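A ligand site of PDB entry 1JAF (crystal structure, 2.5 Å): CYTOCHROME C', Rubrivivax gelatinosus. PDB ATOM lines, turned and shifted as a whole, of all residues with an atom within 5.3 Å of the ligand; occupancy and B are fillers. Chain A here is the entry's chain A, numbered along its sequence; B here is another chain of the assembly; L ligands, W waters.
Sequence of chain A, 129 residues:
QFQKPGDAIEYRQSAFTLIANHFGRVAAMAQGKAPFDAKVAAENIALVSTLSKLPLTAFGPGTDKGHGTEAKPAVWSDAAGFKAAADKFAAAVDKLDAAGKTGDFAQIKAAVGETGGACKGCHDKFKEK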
ATOM      1  N   ILE A   9      -1.462   2.647   0.640  1.00  0.00           N
ATOM      2  CA  ILE A   9      -0.873   3.315  -0.520  1.00  0.00           C
ATOM      3  C   ILE A   9      -1.427   2.778  -1.826  1.00  0.00           C
ATOM      4  O   ILE A   9      -1.817   3.549  -2.697  1.00  0.00           O
ATOM      5  CB  ILE A   9       0.651   3.213  -0.517  1.00  0.00           C
ATOM      6  CG1 ILE A   9       1.202   3.967   0.701  1.00  0.00           C
ATOM      7  CG2 ILE A   9       1.208   3.813  -1.777  1.00  0.00           C
ATOM      8  CD1 ILE A   9       2.689   3.796   0.934  1.00  0.00           C
ATOM      9  N   ARG A  12      -5.241   3.920  -2.174  1.00  0.00           N
ATOM     10  CA  ARG A  12      -5.438   5.287  -2.595  1.00  0.00           C
ATOM     11  C   ARG A  12      -5.006   5.545  -4.042  1.00  0.00           C
ATOM     12  O   ARG A  12      -5.663   6.297  -4.773  1.00  0.00           O
ATOM     13  CB  ARG A  12      -4.774   6.263  -1.626  1.00  0.00           C
ATOM     14  CG  ARG A  12      -3.264   6.210  -1.592  1.00  0.00           C
ATOM     15  CD  ARG A  12      -2.775   6.954  -0.350  1.00  0.00           C
ATOM     16  NE  ARG A  12      -1.335   7.206  -0.363  1.00  0.00           N
ATOM     17  CZ  ARG A  12      -0.595   7.305   0.733  1.00  0.00           C
ATOM     18  NH1 ARG A  12      -1.143   7.171   1.926  1.00  0.00           N
ATOM     19  NH2 ARG A  12       0.702   7.547   0.641  1.00  0.00           N
ATOM     20  N   GLN A  13      -3.917   4.924  -4.462  1.00  0.00           N
ATOM     21  CA  GLN A  13      -3.450   5.102  -5.844  1.00  0.00           C
ATOM     22  C   GLN A  13      -4.488   4.548  -6.829  1.00  0.00           C
ATOM     23  O   GLN A  13      -4.821   5.179  -7.830  1.00  0.00           O
ATOM     24  CB  GLN A  13      -2.094   4.415  -6.037  1.00  0.00           C
ATOM     25  CG  GLN A  13      -0.977   5.021  -5.190  1.00  0.00           C
ATOM     26  CD  GLN A  13       0.394   4.400  -5.452  1.00  0.00           C
ATOM     27  OE1 GLN A  13       0.492   3.281  -5.949  1.00  0.00           O
ATOM     28  NE2 GLN A  13       1.448   5.119  -5.112  1.00  0.00           N
ATOM     29  N   SER A  14      -5.047   3.398  -6.498  1.00  0.00           N
ATOM     30  CA  SER A  14      -6.034   2.754  -7.341  1.00  0.00           C
ATOM     31  C   SER A  14      -7.297   3.577  -7.417  1.00  0.00           C
ATOM     32  O   SER A  14      -7.906   3.695  -8.489  1.00  0.00           O
ATOM     33  CB  SER A  14      -6.341   1.374  -6.791  1.00  0.00           C
ATOM     34  OG  SER A  14      -5.131   0.648  -6.698  1.00  0.00           O
ATOM     35  N   PHE A  16      -7.530   6.858  -7.056  1.00  0.00           N
ATOM     36  CA  PHE A  16      -7.264   8.022  -7.900  1.00  0.00           C
ATOM     37  C   PHE A  16      -7.263   7.662  -9.355  1.00  0.00           C
ATOM     38  O   PHE A  16      -7.827   8.368 -10.182  1.00  0.00           O
ATOM     39  CB  PHE A  16      -5.952   8.687  -7.520  1.00  0.00           C
ATOM     40  CG  PHE A  16      -6.044   9.489  -6.272  1.00  0.00           C
ATOM     41  CD1 PHE A  16      -7.078  10.391  -6.110  1.00  0.00           C
ATOM     42  CD2 PHE A  16      -5.122   9.326  -5.242  1.00  0.00           C
ATOM     43  CE1 PHE A  16      -7.195  11.151  -4.939  1.00  0.00           C
ATOM     44  CE2 PHE A  16      -5.224  10.067  -4.073  1.00  0.00           C
ATOM     45  CZ  PHE A  16      -6.279  10.989  -3.917  1.00  0.00           C
ATOM     46  N   THR A  17      -6.688   6.509  -9.690  1.00  0.00           N
ATOM     47  CA  THR A  17      -6.652   6.042 -11.058  1.00  0.00           C
ATOM     48  C   THR A  17      -8.080   5.893 -11.629  1.00  0.00           C
ATOM     49  O   THR A  17      -8.348   6.312 -12.763  1.00  0.00           O
ATOM     50  CB  THR A  17      -5.935   4.688 -11.132  1.00  0.00           C
ATOM     51  OG1 THR A  17      -4.585   4.851 -10.690  1.00  0.00           O
ATOM     52  CG2 THR A  17      -5.920   4.140 -12.544  1.00  0.00           C
ATOM     53  N   ILE A  19     -10.855   7.398 -10.510  1.00  0.00           N
ATOM     54  CA  ILE A  19     -11.449   8.740 -10.526  1.00  0.00           C
ATOM     55  C   ILE A  19     -10.961   9.496 -11.748  1.00  0.00           C
ATOM     56  O   ILE A  19     -11.736  10.127 -12.462  1.00  0.00           O
ATOM     57  CB  ILE A  19     -11.038   9.525  -9.267  1.00  0.00           C
ATOM     58  CG1 ILE A  19     -11.763   8.936  -8.049  1.00  0.00           C
ATOM     59  CG2 ILE A  19     -11.370  10.981  -9.421  1.00  0.00           C
ATOM     60  CD1 ILE A  19     -11.291   9.501  -6.738  1.00  0.00           C
ATOM     61  N   ALA A  20      -9.666   9.437 -11.994  1.00  0.00           N
ATOM     62  CA  ALA A  20      -9.107  10.111 -13.141  1.00  0.00           C
ATOM     63  C   ALA A  20      -9.773   9.612 -14.415  1.00  0.00           C
ATOM     64  O   ALA A  20     -10.281  10.402 -15.212  1.00  0.00           O
ATOM     65  CB  ALA A  20      -7.610   9.887 -13.223  1.00  0.00           C
ATOM     66  N   PHE A  23     -13.550  10.725 -14.550  1.00  0.00           N
ATOM     67  CA  PHE A  23     -13.711  12.168 -14.573  1.00  0.00           C
ATOM     68  C   PHE A  23     -13.319  12.615 -15.977  1.00  0.00           C
ATOM     69  O   PHE A  23     -13.954  13.497 -16.566  1.00  0.00           O
ATOM     70  CB  PHE A  23     -12.801  12.852 -13.544  1.00  0.00           C
ATOM     71  CG  PHE A  23     -12.814  14.372 -13.616  1.00  0.00           C
ATOM     72  CD1 PHE A  23     -14.006  15.081 -13.477  1.00  0.00           C
ATOM     73  CD2 PHE A  23     -11.645  15.081 -13.842  1.00  0.00           C
ATOM     74  CE1 PHE A  23     -14.031  16.478 -13.567  1.00  0.00           C
ATOM     75  CE2 PHE A  23     -11.657  16.471 -13.930  1.00  0.00           C
ATOM     76  CZ  PHE A  23     -12.854  17.172 -13.790  1.00  0.00           C
ATOM     77  N   LEU A  56      -9.308   9.484   0.373  1.00  0.00           N
ATOM     78  CA  LEU A  56      -8.977  10.375   1.463  1.00  0.00           C
ATOM     79  C   LEU A  56      -8.966   9.723   2.846  1.00  0.00           C
ATOM     80  O   LEU A  56      -8.616  10.372   3.826  1.00  0.00           O
ATOM     81  CB  LEU A  56      -9.855  11.624   1.409  1.00  0.00           C
ATOM     82  CG  LEU A  56      -9.684  12.389   0.086  1.00  0.00           C
ATOM     83  CD1 LEU A  56     -10.740  13.473  -0.051  1.00  0.00           C
ATOM     84  CD2 LEU A  56      -8.268  12.961  -0.050  1.00  0.00           C
ATOM     85  N   PHE A  59      -4.795   7.978   4.049  1.00  0.00           N
ATOM     86  CA  PHE A  59      -3.597   8.804   4.231  1.00  0.00           C
ATOM     87  C   PHE A  59      -3.181   8.860   5.708  1.00  0.00           C
ATOM     88  O   PHE A  59      -2.639   9.854   6.180  1.00  0.00           O
ATOM     89  CB  PHE A  59      -3.840  10.208   3.697  1.00  0.00           C
ATOM     90  CG  PHE A  59      -3.693  10.316   2.206  1.00  0.00           C
ATOM     91  CD1 PHE A  59      -2.444  10.500   1.638  1.00  0.00           C
ATOM     92  CD2 PHE A  59      -4.805  10.247   1.383  1.00  0.00           C
ATOM     93  CE1 PHE A  59      -2.294  10.613   0.262  1.00  0.00           C
ATOM     94  CE2 PHE A  59      -4.667  10.362  -0.008  1.00  0.00           C
ATOM     95  CZ  PHE A  59      -3.406  10.544  -0.561  1.00  0.00           C
ATOM     96  N   GLY A  68       5.947   2.749  -3.803  1.00  0.00           N
ATOM     97  CA  GLY A  68       6.038   3.776  -4.831  1.00  0.00           C
ATOM     98  C   GLY A  68       5.123   4.959  -4.641  1.00  0.00           C
ATOM     99  O   GLY A  68       4.627   5.526  -5.620  1.00  0.00           O
ATOM    100  N   THR A  69       4.901   5.358  -3.389  1.00  0.00           N
ATOM    101  CA  THR A  69       4.028   6.492  -3.097  1.00  0.00           C
ATOM    102  C   THR A  69       4.578   7.804  -3.647  1.00  0.00           C
ATOM    103  O   THR A  69       5.787   8.036  -3.628  1.00  0.00           O
ATOM    104  CB  THR A  69       3.821   6.644  -1.588  1.00  0.00           C
ATOM    105  OG1 THR A  69       2.983   7.773  -1.338  1.00  0.00           O
ATOM    106  CG2 THR A  69       5.149   6.852  -0.887  1.00  0.00           C
ATOM    107  N   GLU A  70       3.682   8.654  -4.129  1.00  0.00           N
ATOM    108  CA  GLU A  70       4.063   9.956  -4.671  1.00  0.00           C
ATOM    109  C   GLU A  70       3.549  11.081  -3.816  1.00  0.00           C
ATOM    110  O   GLU A  70       3.535  12.227  -4.233  1.00  0.00           O
ATOM    111  CB  GLU A  70       3.513  10.131  -6.072  1.00  0.00           C
ATOM    112  CG  GLU A  70       4.197   9.291  -7.097  1.00  0.00           C
ATOM    113  CD  GLU A  70       3.820   9.703  -8.494  1.00  0.00           C
ATOM    114  OE1 GLU A  70       2.745   9.290  -8.961  1.00  0.00           O
ATOM    115  OE2 GLU A  70       4.617  10.435  -9.127  1.00  0.00           O
ATOM    116  N   ALA A  71       3.073  10.753  -2.628  1.00  0.00           N
ATOM    117  CA  ALA A  71       2.537  11.755  -1.718  1.00  0.00           C
ATOM    118  C   ALA A  71       3.685  12.473  -1.039  1.00  0.00           C
ATOM    119  O   ALA A  71       4.522  11.841  -0.390  1.00  0.00           O
ATOM    120  CB  ALA A  71       1.661  11.089  -0.672  1.00  0.00           C
ATOM    121  N   LYS A  72       3.732  13.789  -1.172  1.00  0.00           N
ATOM    122  CA  LYS A  72       4.791  14.543  -0.519  1.00  0.00           C
ATOM    123  C   LYS A  72       4.623  14.517   0.987  1.00  0.00           C
ATOM    124  O   LYS A  72       3.508  14.393   1.504  1.00  0.00           O
ATOM    125  CB  LYS A  72       4.848  15.974  -1.064  1.00  0.00           C
ATOM    126  CG  LYS A  72       5.487  16.049  -2.445  1.00  0.00           C
ATOM    127  CD  LYS A  72       5.918  17.460  -2.833  1.00  0.00           C
ATOM    128  CE  LYS A  72       7.089  17.411  -3.822  1.00  0.00           C
ATOM    129  NZ  LYS A  72       7.470  18.738  -4.401  1.00  0.00           N
ATOM    130  N   VAL A  75       2.093  16.255   3.212  1.00  0.00           N
ATOM    131  CA  VAL A  75       0.775  15.680   3.422  1.00  0.00           C
ATOM    132  C   VAL A  75       0.544  15.489   4.920  1.00  0.00           C
ATOM    133  O   VAL A  75      -0.575  15.599   5.418  1.00  0.00           O
ATOM    134  CB  VAL A  75       0.627  14.320   2.694  1.00  0.00           C
ATOM    135  CG1 VAL A  75      -0.669  13.634   3.082  1.00  0.00           C
ATOM    136  CG2 VAL A  75       0.651  14.515   1.185  1.00  0.00           C
ATOM    137  N   PHE A  82      -3.601  20.089   3.873  1.00  0.00           N
ATOM    138  CA  PHE A  82      -4.162  18.963   3.165  1.00  0.00           C
ATOM    139  C   PHE A  82      -5.670  18.865   3.385  1.00  0.00           C
ATOM    140  O   PHE A  82      -6.408  18.721   2.425  1.00  0.00           O
ATOM    141  CB  PHE A  82      -3.495  17.654   3.569  1.00  0.00           C
ATOM    142  CG  PHE A  82      -3.715  16.536   2.593  1.00  0.00           C
ATOM    143  CD1 PHE A  82      -3.119  16.553   1.344  1.00  0.00           C
ATOM    144  CD2 PHE A  82      -4.501  15.443   2.949  1.00  0.00           C
ATOM    145  CE1 PHE A  82      -3.296  15.507   0.458  1.00  0.00           C
ATOM    146  CE2 PHE A  82      -4.683  14.388   2.066  1.00  0.00           C
ATOM    147  CZ  PHE A  82      -4.076  14.413   0.823  1.00  0.00           C
ATOM    148  N   ALA A  85      -7.253  21.375   1.204  1.00  0.00           N
ATOM    149  CA  ALA A  85      -7.306  20.994  -0.210  1.00  0.00           C
ATOM    150  C   ALA A  85      -8.377  19.920  -0.463  1.00  0.00           C
ATOM    151  O   ALA A  85      -9.051  19.920  -1.496  1.00  0.00           O
ATOM    152  CB  ALA A  85      -5.948  20.473  -0.631  1.00  0.00           C
ATOM    153  N   ALA A  86      -8.516  19.006   0.477  1.00  0.00           N
ATOM    154  CA  ALA A  86      -9.496  17.946   0.397  1.00  0.00           C
ATOM    155  C   ALA A  86     -10.888  18.525   0.502  1.00  0.00           C
ATOM    156  O   ALA A  86     -11.830  18.055  -0.160  1.00  0.00           O
ATOM    157  CB  ALA A  86      -9.272  16.949   1.495  1.00  0.00           C
ATOM    158  N   PHE A  89     -11.919  20.066  -2.781  1.00  0.00           N
ATOM    159  CA  PHE A  89     -12.222  18.988  -3.710  1.00  0.00           C
ATOM    160  C   PHE A  89     -13.628  18.449  -3.474  1.00  0.00           C
ATOM    161  O   PHE A  89     -14.413  18.280  -4.398  1.00  0.00           O
ATOM    162  CB  PHE A  89     -11.193  17.868  -3.543  1.00  0.00           C
ATOM    163  CG  PHE A  89     -11.462  16.660  -4.386  1.00  0.00           C
ATOM    164  CD1 PHE A  89     -11.641  16.803  -5.760  1.00  0.00           C
ATOM    165  CD2 PHE A  89     -11.563  15.405  -3.809  1.00  0.00           C
ATOM    166  CE1 PHE A  89     -11.920  15.692  -6.556  1.00  0.00           C
ATOM    167  CE2 PHE A  89     -11.840  14.284  -4.595  1.00  0.00           C
ATOM    168  CZ  PHE A  89     -12.019  14.428  -5.969  1.00  0.00           C
ATOM    169  N   THR A 115     -13.790  21.245 -10.502  1.00  0.00           N
ATOM    170  CA  THR A 115     -13.231  19.995 -10.027  1.00  0.00           C
ATOM    171  C   THR A 115     -11.782  19.876 -10.526  1.00  0.00           C
ATOM    172  O   THR A 115     -10.862  19.616  -9.742  1.00  0.00           O
ATOM    173  CB  THR A 115     -14.049  18.808 -10.517  1.00  0.00           C
ATOM    174  OG1 THR A 115     -15.410  18.997 -10.110  1.00  0.00           O
ATOM    175  CG2 THR A 115     -13.548  17.514  -9.922  1.00  0.00           C
ATOM    176  N   ALA A 118      -9.489  21.769  -8.559  1.00  0.00           N
ATOM    177  CA  ALA A 118      -9.279  21.199  -7.239  1.00  0.00           C
ATOM    178  C   ALA A 118      -8.276  20.049  -7.276  1.00  0.00           C
ATOM    179  O   ALA A 118      -7.572  19.817  -6.297  1.00  0.00           O
ATOM    180  CB  ALA A 118     -10.587  20.736  -6.670  1.00  0.00           C
ATOM    181  N   CYS A 119      -8.210  19.349  -8.398  1.00  0.00           N
ATOM    182  CA  CYS A 119      -7.277  18.241  -8.528  1.00  0.00           C
ATOM    183  C   CYS A 119      -5.870  18.789  -8.554  1.00  0.00           C
ATOM    184  O   CYS A 119      -5.021  18.372  -7.758  1.00  0.00           O
ATOM    185  CB  CYS A 119      -7.513  17.458  -9.814  1.00  0.00           C
ATOM    186  SG  CYS A 119      -9.182  16.756 -10.021  1.00  0.00           S
ATOM    187  N   CYS A 122      -4.475  20.632  -5.224  1.00  0.00           N
ATOM    188  CA  CYS A 122      -3.934  19.706  -4.236  1.00  0.00           C
ATOM    189  C   CYS A 122      -2.617  19.107  -4.725  1.00  0.00           C
ATOM    190  O   CYS A 122      -1.646  19.062  -3.983  1.00  0.00           O
ATOM    191  CB  CYS A 122      -4.918  18.587  -3.941  1.00  0.00           C
ATOM    192  SG  CYS A 122      -4.300  17.470  -2.637  1.00  0.00           S
ATOM    193  N   HIS A 123      -2.583  18.702  -5.992  1.00  0.00           N
ATOM    194  CA  HIS A 123      -1.382  18.113  -6.565  1.00  0.00           C
ATOM    195  C   HIS A 123      -0.157  18.991  -6.478  1.00  0.00           C
ATOM    196  O   HIS A 123       0.930  18.496  -6.162  1.00  0.00           O
ATOM    197  CB  HIS A 123      -1.596  17.706  -8.019  1.00  0.00           C
ATOM    198  CG  HIS A 123      -2.340  16.413  -8.179  1.00  0.00           C
ATOM    199  ND1 HIS A 123      -2.334  15.759  -9.402  1.00  0.00           N
ATOM    200  CD2 HIS A 123      -3.127  15.786  -7.215  1.00  0.00           C
ATOM    201  CE1 HIS A 123      -3.178  14.732  -9.159  1.00  0.00           C
ATOM    202  NE2 HIS A 123      -3.624  14.696  -7.932  1.00  0.00           N
ATOM    203  N   PHE A 126       0.852  18.914  -2.717  1.00  0.00           N
ATOM    204  CA  PHE A 126       1.139  17.640  -2.086  1.00  0.00           C
ATOM    205  C   PHE A 126       1.514  16.416  -2.917  1.00  0.00           C
ATOM    206  O   PHE A 126       1.584  15.316  -2.357  1.00  0.00           O
ATOM    207  CB  PHE A 126      -0.034  17.241  -1.203  1.00  0.00           C
ATOM    208  CG  PHE A 126      -0.462  18.326  -0.255  1.00  0.00           C
ATOM    209  CD1 PHE A 126       0.256  18.558   0.915  1.00  0.00           C
ATOM    210  CD2 PHE A 126      -1.602  19.060  -0.496  1.00  0.00           C
ATOM    211  CE1 PHE A 126      -0.169  19.528   1.820  1.00  0.00           C
ATOM    212  CE2 PHE A 126      -2.027  20.030   0.409  1.00  0.00           C
ATOM    213  CZ  PHE A 126      -1.320  20.254   1.574  1.00  0.00           C
ATOM    214  N   LYS A 127       1.798  16.555  -4.217  1.00  0.00           N
ATOM    215  CA  LYS A 127       2.114  15.370  -5.008  1.00  0.00           C
ATOM    216  C   LYS A 127       3.417  15.412  -5.808  1.00  0.00           C
ATOM    217  O   LYS A 127       3.819  16.457  -6.296  1.00  0.00           O
ATOM    218  CB  LYS A 127       0.953  15.043  -5.953  1.00  0.00           C
ATOM    219  CG  LYS A 127       1.154  13.800  -6.824  1.00  0.00           C
ATOM    220  CD  LYS A 127       0.096  13.706  -7.904  1.00  0.00           C
ATOM    221  CE  LYS A 127       0.267  12.490  -8.813  1.00  0.00           C
ATOM    222  NZ  LYS A 127       1.535  12.443  -9.582  1.00  0.00           N
ATOM    223  N   GLU B  10      -3.699  -0.717 -15.912  1.00  0.00           N
ATOM    224  CA  GLU B  10      -3.738  -0.001 -14.640  1.00  0.00           C
ATOM    225  C   GLU B  10      -5.140   0.152 -14.099  1.00  0.00           C
ATOM    226  O   GLU B  10      -5.366   0.060 -12.906  1.00  0.00           O
ATOM    227  CB  GLU B  10      -3.134   1.381 -14.784  1.00  0.00           C
ATOM    228  CG  GLU B  10      -1.632   1.408 -14.721  1.00  0.00           C
ATOM    229  CD  GLU B  10      -1.141   2.702 -14.103  1.00  0.00           C
ATOM    230  OE1 GLU B  10      -1.084   2.774 -12.862  1.00  0.00           O
ATOM    231  OE2 GLU B  10      -0.837   3.651 -14.874  1.00  0.00           O
HETATM  232  C1  LIG L   1      -2.351  10.702  -7.026  1.00  0.00           C
HETATM  233  C2  LIG L   1      -5.692  12.097 -10.109  1.00  0.00           C
HETATM  234  C3  LIG L   1      -7.584  14.877  -6.794  1.00  0.00           C
HETATM  235  C4  LIG L   1      -3.881  14.019  -3.917  1.00  0.00           C
HETATM  236  C5  LIG L   1      -3.162  10.797  -8.116  1.00  0.00           C
HETATM  237  C6  LIG L   1      -3.025   9.960  -9.288  1.00  0.00           C
HETATM  238  C7  LIG L   1      -3.940  10.396 -10.171  1.00  0.00           C
HETATM  239  C8  LIG L   1      -4.627  11.489  -9.529  1.00  0.00           C
HETATM  240  C9  LIG L   1      -4.193   9.784 -11.526  1.00  0.00           C
HETATM  241  C10 LIG L   1      -2.023   8.877  -9.629  1.00  0.00           C
HETATM  242  C11 LIG L   1      -2.177   7.560  -8.911  1.00  0.00           C
HETATM  243  C12 LIG L   1      -1.143   6.543  -9.335  1.00  0.00           C
HETATM  244  O1  LIG L   1       0.060   6.853  -9.249  1.00  0.00           O
HETATM  245  O2  LIG L   1      -1.532   5.436  -9.753  1.00  0.00           O
HETATM  246  C13 LIG L   1      -6.483  13.016  -9.494  1.00  0.00           C
HETATM  247  C14 LIG L   1      -7.694  13.556 -10.080  1.00  0.00           C
HETATM  248  C15 LIG L   1      -8.265  14.314  -9.119  1.00  0.00           C
HETATM  249  C16 LIG L   1      -7.371  14.232  -7.965  1.00  0.00           C
HETATM  250  C17 LIG L   1      -8.194  13.395 -11.500  1.00  0.00           C
HETATM  251  C18 LIG L   1      -9.469  15.248  -9.100  1.00  0.00           C
HETATM  252  C19 LIG L   1     -10.755  14.627  -9.653  1.00  0.00           C
HETATM  253  C20 LIG L   1      -6.726  14.930  -5.750  1.00  0.00           C
HETATM  254  C21 LIG L   1      -6.969  15.772  -4.581  1.00  0.00           C
HETATM  255  C22 LIG L   1      -5.939  15.557  -3.726  1.00  0.00           C
HETATM  256  C23 LIG L   1      -5.048  14.592  -4.429  1.00  0.00           C
HETATM  257  C24 LIG L   1      -8.127  16.751  -4.346  1.00  0.00           C
HETATM  258  C25 LIG L   1      -5.513  16.219  -2.390  1.00  0.00           C
HETATM  259  C26 LIG L   1      -6.522  16.753  -1.382  1.00  0.00           C
HETATM  260  C27 LIG L   1      -3.102  13.067  -4.552  1.00  0.00           C
HETATM  261  C28 LIG L   1      -1.930  12.422  -3.961  1.00  0.00           C
HETATM  262  C29 LIG L   1      -1.569  11.430  -4.802  1.00  0.00           C
HETATM  263  C30 LIG L   1      -2.446  11.520  -5.943  1.00  0.00           C
HETATM  264  C31 LIG L   1      -1.153  12.821  -2.740  1.00  0.00           C
HETATM  265  C32 LIG L   1      -0.481  10.410  -4.580  1.00  0.00           C
HETATM  266  C33 LIG L   1      -0.914   9.131  -3.913  1.00  0.00           C
HETATM  267  C34 LIG L   1       0.247   8.190  -3.690  1.00  0.00           C
HETATM  268  O3  LIG L   1       0.446   7.740  -2.541  1.00  0.00           O
HETATM  269  O4  LIG L   1       0.991   7.917  -4.654  1.00  0.00           O
HETATM  270  N1  LIG L   1      -4.147  11.751  -8.275  1.00  0.00           N
HETATM  271  N2  LIG L   1      -6.271  13.459  -8.205  1.00  0.00           N
HETATM  272  N3  LIG L   1      -5.527  14.258  -5.693  1.00  0.00           N
HETATM  273  N4  LIG L   1      -3.388  12.523  -5.793  1.00  0.00           N
HETATM  274 FE1  LIG L   1      -4.706  13.178  -7.084  1.00  0.00          FE
HETATM  275  O   HOH W   1       0.027   2.966  -9.582  1.00  0.00           O
HETATM  276  O   HOH W   2       0.685   8.374  -7.226  1.00  0.00           O
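An oxygen (O3) of the ligand sits at hydrogen-bond distance from the side-chain hydroxyl of Thr 69.
C18 of the ligand is bonded to SG of Cys 119 (1.8 Å).
An oxygen (O2) of the ligand is in hydrogen-bond range of the side-chain hydroxyl of Thr 17 (3.2 Å).
The guanidinium group (NE) of Arg 12 lies within salt-bridge range of an oxygen (O3) of the ligand, at 2.9 Å.
An oxygen (O4) of the ligand sits at hydrogen-bond distance from the backbone NH of Glu 70, at 2.8 Å.
An iron atom (FE1) of the ligand is bound by a ring nitrogen (NE2) of His 123, at 2.0 Å.
O4 of the ligand sits at hydrogen-bond distance from NE2 of Gln 13, 2.9 Å away.
The side-chain sulfur (SG) of Cys 122 is bonded to a carbon (C25) of the ligand (1.8 Å).
Water W2 bridges an oxygen (O1) of the ligand (2.6 Å) and the side-chain carboxylate (OE1) of Glu 70 (2.8 Å).
Water W1 lies within hydrogen-bond range of O2 of the ligand and OE1 of Glu 10 of chain B.
The backbone carbonyl oxygen of Gln 13 sits at hydrogen-bond distance from the side-chain hydroxyl of Thr 17, at 2.9 Å.
NE2 of Gln 13 is in hydrogen-bond range of O of Gly 68 (3.2 Å).
The backbone NH of Lys 72 is in hydrogen-bond range of the backbone carbonyl oxygen of Phe 126 (2.9 Å).
OG1 of Thr 69 is in hydrogen-bond range of N of Ala 71, at 3.2 Å.
The side-chain hydroxyl (OG1) of Thr 69 is in hydrogen-bond range of the guanidinium group (NH2) of Arg 12 (3.0 Å).
The side-chain carboxylate (OE1) of Glu 70 lies within salt-bridge range of the side-chain amino group (NZ) of Lys 127 (3.4 Å).
Phe 16 touches the ligand (CE2 to N4, 3.5 Å).
Ile 19 touches the ligand (CG2 to C19, 3.7 Å).
Ala 20 touches the ligand (CA to C17, 3.8 Å).
CZ of Phe 59 touches C31 of the ligand, at 3.9 Å.
CB of Ala 71 touches C31 of the ligand, 3.9 Å away.
Phe 82 touches the ligand.
C of Ala 85 touches C26 of the ligand, 3.8 Å away.
Ala 86 touches the ligand (N to C26, 3.5 Å).
Phe 89 touches the ligand.
Ala 118 touches the ligand (O to C24, 3.7 Å).
Phe 126 touches the ligand.
CE of Lys 127 touches C1 of the ligand, at 3.6 Å.
20 residues have an atom within 4 Å of the ligand: Arg 12, Gln 13, Phe 16, Thr 17, Ile 19, Ala 20, Phe 59, Thr 69, Glu 70, Ala 71, Phe 82, Ala 85, Ala 86, Phe 89, Ala 118, Cys 119, Cys 122, His 123, Phe 126 and Lys 127.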
